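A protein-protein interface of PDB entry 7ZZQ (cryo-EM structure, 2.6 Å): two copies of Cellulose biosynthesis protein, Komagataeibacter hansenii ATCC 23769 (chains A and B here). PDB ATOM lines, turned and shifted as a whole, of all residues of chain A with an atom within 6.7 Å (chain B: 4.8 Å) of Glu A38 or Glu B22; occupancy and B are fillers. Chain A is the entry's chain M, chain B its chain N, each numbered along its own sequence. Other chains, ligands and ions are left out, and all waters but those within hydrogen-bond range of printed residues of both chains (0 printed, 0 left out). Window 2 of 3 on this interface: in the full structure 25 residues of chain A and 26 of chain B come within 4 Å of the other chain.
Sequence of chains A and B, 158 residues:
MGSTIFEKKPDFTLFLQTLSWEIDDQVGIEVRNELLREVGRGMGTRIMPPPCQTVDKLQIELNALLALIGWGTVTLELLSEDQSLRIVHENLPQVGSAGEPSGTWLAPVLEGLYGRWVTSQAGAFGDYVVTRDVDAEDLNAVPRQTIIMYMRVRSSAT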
ATOM      1  N   VAL A  31       3.730 -23.119 -25.281  1.00  0.00           N
ATOM      2  CA  VAL A  31       2.457 -23.587 -25.823  1.00  0.00           C
ATOM      3  C   VAL A  31       1.964 -24.795 -25.037  1.00  0.00           C
ATOM      4  O   VAL A  31       0.774 -24.901 -24.711  1.00  0.00           O
ATOM      5  CB  VAL A  31       2.601 -23.904 -27.323  1.00  0.00           C
ATOM      6  CG1 VAL A  31       1.273 -24.357 -27.904  1.00  0.00           C
ATOM      7  CG2 VAL A  31       3.129 -22.692 -28.069  1.00  0.00           C
ATOM      8  N   ASN A  33       2.711 -25.481 -21.924  1.00  0.00           N
ATOM      9  CA  ASN A  33       2.302 -25.005 -20.606  1.00  0.00           C
ATOM     10  C   ASN A  33       0.915 -24.374 -20.649  1.00  0.00           C
ATOM     11  O   ASN A  33       0.095 -24.606 -19.755  1.00  0.00           O
ATOM     12  CB  ASN A  33       3.327 -24.009 -20.065  1.00  0.00           C
ATOM     13  CG  ASN A  33       4.548 -24.690 -19.483  1.00  0.00           C
ATOM     14  OD1 ASN A  33       4.531 -25.887 -19.203  1.00  0.00           O
ATOM     15  ND2 ASN A  33       5.615 -23.926 -19.290  1.00  0.00           N
ATOM     16  N   GLU A  34       0.636 -23.570 -21.677  1.00  0.00           N
ATOM     17  CA  GLU A  34      -0.686 -22.960 -21.792  1.00  0.00           C
ATOM     18  C   GLU A  34      -1.766 -24.013 -22.017  1.00  0.00           C
ATOM     19  O   GLU A  34      -2.854 -23.933 -21.433  1.00  0.00           O
ATOM     20  CB  GLU A  34      -0.692 -21.932 -22.923  1.00  0.00           C
ATOM     21  CG  GLU A  34      -1.786 -20.874 -22.815  1.00  0.00           C
ATOM     22  CD  GLU A  34      -2.201 -20.587 -21.380  1.00  0.00           C
ATOM     23  OE1 GLU A  34      -1.545 -19.748 -20.727  1.00  0.00           O
ATOM     24  OE2 GLU A  34      -3.196 -21.181 -20.913  1.00  0.00           O
ATOM     25  N   LEU A  35      -1.481 -25.013 -22.855  1.00  0.00           N
ATOM     26  CA  LEU A  35      -2.448 -26.081 -23.080  1.00  0.00           C
ATOM     27  C   LEU A  35      -2.717 -26.861 -21.799  1.00  0.00           C
ATOM     28  O   LEU A  35      -3.866 -27.198 -21.497  1.00  0.00           O
ATOM     29  CB  LEU A  35      -1.953 -27.013 -24.186  1.00  0.00           C
ATOM     30  CG  LEU A  35      -2.746 -28.305 -24.391  1.00  0.00           C
ATOM     31  CD1 LEU A  35      -4.098 -28.010 -25.021  1.00  0.00           C
ATOM     32  CD2 LEU A  35      -1.959 -29.288 -25.236  1.00  0.00           C
ATOM     33  N   LEU A  36      -1.667 -27.145 -21.025  1.00  0.00           N
ATOM     34  CA  LEU A  36      -1.852 -27.877 -19.777  1.00  0.00           C
ATOM     35  C   LEU A  36      -2.579 -27.040 -18.730  1.00  0.00           C
ATOM     36  O   LEU A  36      -3.352 -27.584 -17.936  1.00  0.00           O
ATOM     37  CB  LEU A  36      -0.501 -28.355 -19.249  1.00  0.00           C
ATOM     38  CG  LEU A  36       0.111 -29.502 -20.055  1.00  0.00           C
ATOM     39  CD1 LEU A  36       1.492 -29.850 -19.540  1.00  0.00           C
ATOM     40  CD2 LEU A  36      -0.797 -30.719 -20.026  1.00  0.00           C
ATOM     41  N   ARG A  37      -2.354 -25.723 -18.714  1.00  0.00           N
ATOM     42  CA  ARG A  37      -3.125 -24.857 -17.828  1.00  0.00           C
ATOM     43  C   ARG A  37      -4.598 -24.852 -18.211  1.00  0.00           C
ATOM     44  O   ARG A  37      -5.475 -24.868 -17.339  1.00  0.00           O
ATOM     45  CB  ARG A  37      -2.559 -23.439 -17.850  1.00  0.00           C
ATOM     46  CG  ARG A  37      -1.220 -23.305 -17.157  1.00  0.00           C
ATOM     47  CD  ARG A  37      -0.758 -21.863 -17.101  1.00  0.00           C
ATOM     48  NE  ARG A  37       0.685 -21.778 -16.919  1.00  0.00           N
ATOM     49  CZ  ARG A  37       1.544 -21.463 -17.878  1.00  0.00           C
ATOM     50  NH1 ARG A  37       1.137 -21.177 -19.103  1.00  0.00           N
ATOM     51  NH2 ARG A  37       2.843 -21.434 -17.601  1.00  0.00           N
ATOM     52  N   GLU A  38      -4.891 -24.825 -19.514  1.00  0.00           N
ATOM     53  CA  GLU A  38      -6.279 -24.921 -19.959  1.00  0.00           C
ATOM     54  C   GLU A  38      -6.895 -26.254 -19.551  1.00  0.00           C
ATOM     55  O   GLU A  38      -8.059 -26.311 -19.134  1.00  0.00           O
ATOM     56  CB  GLU A  38      -6.358 -24.738 -21.474  1.00  0.00           C
ATOM     57  CG  GLU A  38      -6.653 -23.317 -21.917  1.00  0.00           C
ATOM     58  CD  GLU A  38      -5.790 -22.882 -23.086  1.00  0.00           C
ATOM     59  OE1 GLU A  38      -5.156 -23.754 -23.715  1.00  0.00           O
ATOM     60  OE2 GLU A  38      -5.749 -21.668 -23.378  1.00  0.00           O
ATOM     61  N   VAL A  39      -6.129 -27.339 -19.676  1.00  0.00           N
ATOM     62  CA  VAL A  39      -6.621 -28.654 -19.271  1.00  0.00           C
ATOM     63  C   VAL A  39      -6.909 -28.680 -17.775  1.00  0.00           C
ATOM     64  O   VAL A  39      -7.923 -29.232 -17.336  1.00  0.00           O
ATOM     65  CB  VAL A  39      -5.617 -29.750 -19.676  1.00  0.00           C
ATOM     66  CG1 VAL A  39      -5.978 -31.074 -19.024  1.00  0.00           C
ATOM     67  CG2 VAL A  39      -5.580 -29.898 -21.185  1.00  0.00           C
ATOM     68  N   GLY A  40      -6.024 -28.092 -16.970  1.00  0.00           N
ATOM     69  CA  GLY A  40      -6.272 -28.022 -15.539  1.00  0.00           C
ATOM     70  C   GLY A  40      -7.499 -27.199 -15.195  1.00  0.00           C
ATOM     71  O   GLY A  40      -8.277 -27.564 -14.309  1.00  0.00           O
ATOM     72  N   ARG A  41      -7.687 -26.074 -15.889  1.00  0.00           N
ATOM     73  CA  ARG A  41      -8.878 -25.259 -15.675  1.00  0.00           C
ATOM     74  C   ARG A  41     -10.143 -26.036 -16.012  1.00  0.00           C
ATOM     75  O   ARG A  41     -11.138 -25.966 -15.281  1.00  0.00           O
ATOM     76  CB  ARG A  41      -8.799 -23.983 -16.510  1.00  0.00           C
ATOM     77  CG  ARG A  41      -8.316 -22.768 -15.747  1.00  0.00           C
ATOM     78  CD  ARG A  41      -7.998 -21.621 -16.688  1.00  0.00           C
ATOM     79  NE  ARG A  41      -6.590 -21.247 -16.649  1.00  0.00           N
ATOM     80  CZ  ARG A  41      -5.823 -21.100 -17.721  1.00  0.00           C
ATOM     81  NH1 ARG A  41      -6.294 -21.302 -18.940  1.00  0.00           N
ATOM     82  NH2 ARG A  41      -4.554 -20.738 -17.565  1.00  0.00           N
ATOM     83  N   GLY A  42     -10.127 -26.778 -17.122  1.00  0.00           N
ATOM     84  CA  GLY A  42     -11.269 -27.614 -17.455  1.00  0.00           C
ATOM     85  C   GLY A  42     -11.489 -28.725 -16.446  1.00  0.00           C
ATOM     86  O   GLY A  42     -12.627 -29.099 -16.156  1.00  0.00           O
ATOM     87  N   MET A  43     -10.398 -29.277 -15.909  1.00  0.00           N
ATOM     88  CA  MET A  43     -10.500 -30.279 -14.855  1.00  0.00           C
ATOM     89  C   MET A  43     -11.145 -29.699 -13.607  1.00  0.00           C
ATOM     90  O   MET A  43     -11.865 -30.406 -12.891  1.00  0.00           O
ATOM     91  CB  MET A  43      -9.112 -30.828 -14.527  1.00  0.00           C
ATOM     92  CG  MET A  43      -8.845 -32.225 -15.048  1.00  0.00           C
ATOM     93  SD  MET A  43      -7.142 -32.752 -14.774  1.00  0.00           S
ATOM     94  CE  MET A  43      -7.253 -33.431 -13.123  1.00  0.00           C
ATOM     95  N   ARG A  46     -14.998 -29.841 -13.524  1.00  0.00           N
ATOM     96  CA  ARG A  46     -15.632 -31.143 -13.359  1.00  0.00           C
ATOM     97  C   ARG A  46     -15.655 -31.612 -11.912  1.00  0.00           C
ATOM     98  O   ARG A  46     -16.636 -32.223 -11.482  1.00  0.00           O
ATOM     99  CB  ARG A  46     -14.924 -32.184 -14.230  1.00  0.00           C
ATOM    100  CG  ARG A  46     -14.913 -31.826 -15.704  1.00  0.00           C
ATOM    101  CD  ARG A  46     -14.426 -32.977 -16.562  1.00  0.00           C
ATOM    102  NE  ARG A  46     -14.302 -32.587 -17.961  1.00  0.00           N
ATOM    103  CZ  ARG A  46     -14.467 -33.411 -18.986  1.00  0.00           C
ATOM    104  NH1 ARG A  46     -14.768 -34.685 -18.805  1.00  0.00           N
ATOM    105  NH2 ARG A  46     -14.330 -32.943 -20.223  1.00  0.00           N
ATOM    106  N   PRO A 108       1.707 -27.274 -14.859  1.00  0.00           N
ATOM    107  CA  PRO A 108       0.692 -26.307 -15.318  1.00  0.00           C
ATOM    108  C   PRO A 108      -0.730 -26.799 -15.115  1.00  0.00           C
ATOM    109  O   PRO A 108      -1.645 -25.986 -14.920  1.00  0.00           O
ATOM    110  CB  PRO A 108       1.009 -26.116 -16.809  1.00  0.00           C
ATOM    111  CG  PRO A 108       2.196 -26.938 -17.111  1.00  0.00           C
ATOM    112  CD  PRO A 108       2.778 -27.462 -15.854  1.00  0.00           C
ATOM    113  N   VAL A 109      -0.940 -28.117 -15.165  1.00  0.00           N
ATOM    114  CA  VAL A 109      -2.245 -28.673 -14.823  1.00  0.00           C
ATOM    115  C   VAL A 109      -2.607 -28.313 -13.391  1.00  0.00           C
ATOM    116  O   VAL A 109      -3.744 -27.929 -13.102  1.00  0.00           O
ATOM    117  CB  VAL A 109      -2.256 -30.196 -15.045  1.00  0.00           C
ATOM    118  CG1 VAL A 109      -3.655 -30.752 -14.843  1.00  0.00           C
ATOM    119  CG2 VAL A 109      -1.734 -30.537 -16.431  1.00  0.00           C
ATOM    120  N   GLY A 112      -3.600 -24.518 -13.264  1.00  0.00           N
ATOM    121  CA  GLY A 112      -4.984 -24.283 -13.654  1.00  0.00           C
ATOM    122  C   GLY A 112      -5.982 -24.853 -12.663  1.00  0.00           C
ATOM    123  O   GLY A 112      -6.997 -24.219 -12.349  1.00  0.00           O
ATOM    124  N   ARG A 116      -8.656 -22.588 -10.567  1.00  0.00           N
ATOM    125  CA  ARG A 116     -10.100 -22.789 -10.613  1.00  0.00           C
ATOM    126  C   ARG A 116     -10.663 -23.162  -9.245  1.00  0.00           C
ATOM    127  O   ARG A 116     -11.749 -22.706  -8.875  1.00  0.00           O
ATOM    128  CB  ARG A 116     -10.445 -23.862 -11.645  1.00  0.00           C
ATOM    129  CG  ARG A 116     -11.927 -23.965 -11.953  1.00  0.00           C
ATOM    130  CD  ARG A 116     -12.423 -22.739 -12.697  1.00  0.00           C
ATOM    131  NE  ARG A 116     -12.773 -23.043 -14.080  1.00  0.00           N
ATOM    132  CZ  ARG A 116     -12.495 -22.258 -15.112  1.00  0.00           C
ATOM    133  NH1 ARG A 116     -11.859 -21.108 -14.955  1.00  0.00           N
ATOM    134  NH2 ARG A 116     -12.867 -22.635 -16.332  1.00  0.00           N
ATOM    135  N   THR B  18     -10.585 -34.559 -19.788  1.00  0.00           N
ATOM    136  CA  THR B  18     -10.460 -33.120 -19.994  1.00  0.00           C
ATOM    137  C   THR B  18      -9.478 -32.804 -21.116  1.00  0.00           C
ATOM    138  O   THR B  18      -9.701 -31.875 -21.899  1.00  0.00           O
ATOM    139  CB  THR B  18     -10.029 -32.438 -18.697  1.00  0.00           C
ATOM    140  OG1 THR B  18     -10.785 -32.969 -17.603  1.00  0.00           O
ATOM    141  CG2 THR B  18     -10.268 -30.946 -18.791  1.00  0.00           C
ATOM    142  N   LEU B  19      -8.381 -33.559 -21.203  1.00  0.00           N
ATOM    143  CA  LEU B  19      -7.399 -33.328 -22.253  1.00  0.00           C
ATOM    144  C   LEU B  19      -7.982 -33.612 -23.630  1.00  0.00           C
ATOM    145  O   LEU B  19      -7.743 -32.855 -24.576  1.00  0.00           O
ATOM    146  CB  LEU B  19      -6.160 -34.189 -22.007  1.00  0.00           C
ATOM    147  CG  LEU B  19      -5.028 -34.078 -23.027  1.00  0.00           C
ATOM    148  CD1 LEU B  19      -4.106 -32.923 -22.683  1.00  0.00           C
ATOM    149  CD2 LEU B  19      -4.255 -35.380 -23.104  1.00  0.00           C
ATOM    150  N   SER B  20      -8.741 -34.701 -23.765  1.00  0.00           N
ATOM    151  CA  SER B  20      -9.394 -34.995 -25.035  1.00  0.00           C
ATOM    152  C   SER B  20     -10.395 -33.909 -25.400  1.00  0.00           C
ATOM    153  O   SER B  20     -10.440 -33.460 -26.551  1.00  0.00           O
ATOM    154  CB  SER B  20     -10.081 -36.358 -24.967  1.00  0.00           C
ATOM    155  OG  SER B  20     -10.852 -36.483 -23.788  1.00  0.00           O
ATOM    156  N   TRP B  21     -11.198 -33.466 -24.427  1.00  0.00           N
ATOM    157  CA  TRP B  21     -12.136 -32.375 -24.677  1.00  0.00           C
ATOM    158  C   TRP B  21     -11.409 -31.130 -25.174  1.00  0.00           C
ATOM    159  O   TRP B  21     -11.780 -30.546 -26.201  1.00  0.00           O
ATOM    160  CB  TRP B  21     -12.915 -32.064 -23.398  1.00  0.00           C
ATOM    161  CG  TRP B  21     -14.310 -31.567 -23.621  1.00  0.00           C
ATOM    162  CD1 TRP B  21     -14.716 -30.266 -23.671  1.00  0.00           C
ATOM    163  CD2 TRP B  21     -15.488 -32.363 -23.790  1.00  0.00           C
ATOM    164  NE1 TRP B  21     -16.072 -30.202 -23.877  1.00  0.00           N
ATOM    165  CE2 TRP B  21     -16.570 -31.476 -23.953  1.00  0.00           C
ATOM    166  CE3 TRP B  21     -15.732 -33.738 -23.827  1.00  0.00           C
ATOM    167  CZ2 TRP B  21     -17.875 -31.919 -24.148  1.00  0.00           C
ATOM    168  CZ3 TRP B  21     -17.028 -34.175 -24.022  1.00  0.00           C
ATOM    169  CH2 TRP B  21     -18.083 -33.269 -24.179  1.00  0.00           C
ATOM    170  N   GLU B  22     -10.352 -30.726 -24.468  1.00  0.00           N
ATOM    171  CA  GLU B  22      -9.626 -29.512 -24.824  1.00  0.00           C
ATOM    172  C   GLU B  22      -8.978 -29.637 -26.198  1.00  0.00           C
ATOM    173  O   GLU B  22      -9.083 -28.728 -27.030  1.00  0.00           O
ATOM    174  CB  GLU B  22      -8.573 -29.211 -23.755  1.00  0.00           C
ATOM    175  CG  GLU B  22      -8.023 -27.796 -23.790  1.00  0.00           C
ATOM    176  CD  GLU B  22      -9.080 -26.750 -23.501  1.00  0.00           C
ATOM    177  OE1 GLU B  22      -9.787 -26.887 -22.479  1.00  0.00           O
ATOM    178  OE2 GLU B  22      -9.206 -25.793 -24.293  1.00  0.00           O
ATOM    179  N   ILE B  23      -8.308 -30.763 -26.456  1.00  0.00           N
ATOM    180  CA  ILE B  23      -7.611 -30.945 -27.726  1.00  0.00           C
ATOM    181  C   ILE B  23      -8.600 -30.941 -28.883  1.00  0.00           C
ATOM    182  O   ILE B  23      -8.375 -30.285 -29.906  1.00  0.00           O
ATOM    183  CB  ILE B  23      -6.771 -32.236 -27.695  1.00  0.00           C
ATOM    184  CG1 ILE B  23      -5.535 -32.044 -26.816  1.00  0.00           C
ATOM    185  CG2 ILE B  23      -6.358 -32.645 -29.097  1.00  0.00           C
ATOM    186  CD1 ILE B  23      -4.710 -33.295 -26.648  1.00  0.00           C
ATOM    187  N   ASP B  24      -9.718 -31.658 -28.738  1.00  0.00           N
ATOM    188  CA  ASP B  24     -10.736 -31.634 -29.781  1.00  0.00           C
ATOM    189  C   ASP B  24     -11.322 -30.239 -29.954  1.00  0.00           C
ATOM    190  O   ASP B  24     -11.736 -29.873 -31.059  1.00  0.00           O
ATOM    191  CB  ASP B  24     -11.838 -32.643 -29.460  1.00  0.00           C
ATOM    192  CG  ASP B  24     -11.369 -34.076 -29.600  1.00  0.00           C
ATOM    193  OD1 ASP B  24     -10.142 -34.300 -29.624  1.00  0.00           O
ATOM    194  OD2 ASP B  24     -12.227 -34.979 -29.683  1.00  0.00           O
ATOM    195  N   ASP B  25     -11.365 -29.449 -28.878  1.00  0.00           N
ATOM    196  CA  ASP B  25     -11.880 -28.087 -28.984  1.00  0.00           C
ATOM    197  C   ASP B  25     -10.944 -27.194 -29.791  1.00  0.00           C
ATOM    198  O   ASP B  25     -11.385 -26.475 -30.694  1.00  0.00           O
ATOM    199  CB  ASP B  25     -12.109 -27.508 -27.588  1.00  0.00           C
ATOM    200  CG  ASP B  25     -13.379 -26.689 -27.499  1.00  0.00           C
ATOM    201  OD1 ASP B  25     -14.380 -27.199 -26.953  1.00  0.00           O
ATOM    202  OD2 ASP B  25     -13.378 -25.534 -27.974  1.00  0.00           O
ATOM    203  N   GLN B  26      -9.644 -27.222 -29.482  1.00  0.00           N
ATOM    204  CA  GLN B  26      -8.733 -26.279 -30.130  1.00  0.00           C
ATOM    205  C   GLN B  26      -8.325 -26.742 -31.525  1.00  0.00           C
ATOM    206  O   GLN B  26      -8.440 -25.981 -32.492  1.00  0.00           O
ATOM    207  CB  GLN B  26      -7.495 -26.037 -29.262  1.00  0.00           C
ATOM    208  CG  GLN B  26      -7.731 -26.157 -27.773  1.00  0.00           C
ATOM    209  CD  GLN B  26      -6.732 -25.366 -26.954  1.00  0.00           C
ATOM    210  OE1 GLN B  26      -5.710 -24.913 -27.466  1.00  0.00           O
ATOM    211  NE2 GLN B  26      -7.024 -25.194 -25.671  1.00  0.00           N
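The side-chain amide nitrogen of Gln B26 sits at hydrogen-bond distance from the side-chain carboxylate of Glu A38, at 3.1 Å.
Val A31 touches none of the printed residues of chain B. Arg A37 touches none of the printed residues of chain B. Of chain B, only Glu B22 and Gln B26 come within 4 Å of Glu A38. Printed residues of chain B within 4 Å of Met A43: Thr B18. Of the printed residues of chain B, Arg A46 touches Thr B18 and Trp B21. Printed residues of chain A within 4 Å of Glu B22: Glu A38 (3.8 Å). The nearest printed residue of chain B that does not touch Glu A38 is Thr B18 (5.1 Å). The nearest printed residue of chain A that does not touch Glu B22 is Val A39 (4.004 Å). The nearest printed residue of chain B that does not touch Val A39 is Glu B22 (4.004 Å).
Among the printed residues, pairs that only touch across the chains: Val A39 with Thr B18 (3.2 Å), Met A43 with Thr B18 (3.3 Å), Gly A42 with Thr B18 (3.5 Å), Arg A46 with Thr B18 (3.6 Å), Arg A46 with Trp B21 (3.6 Å), Val A39 with Leu B19 (3.7 Å) and Glu A38 with Glu B22 (3.8 Å).
No position is printed for both chains. Of the 8 pairs that touch across the chains among the printed residues, none has its exchanged pair printed and touching as well.
Hydrophobic or aromatic side chains of chain B within 4 Å of the printed part of chain A: Leu B19 and Trp B21. Hydrophobic or aromatic side chains of chain A that line the printed part of chain B: Val A39 and Met A43. Among the printed residues, no Asp or Glu carboxylate lies within 4 Å of a Lys or Arg side-chain nitrogen of the other chain.
The side-chain carboxylate (OE2) of Glu B22 is in hydrogen-bond range of the side-chain amide nitrogen (NE2) of Gln B26.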
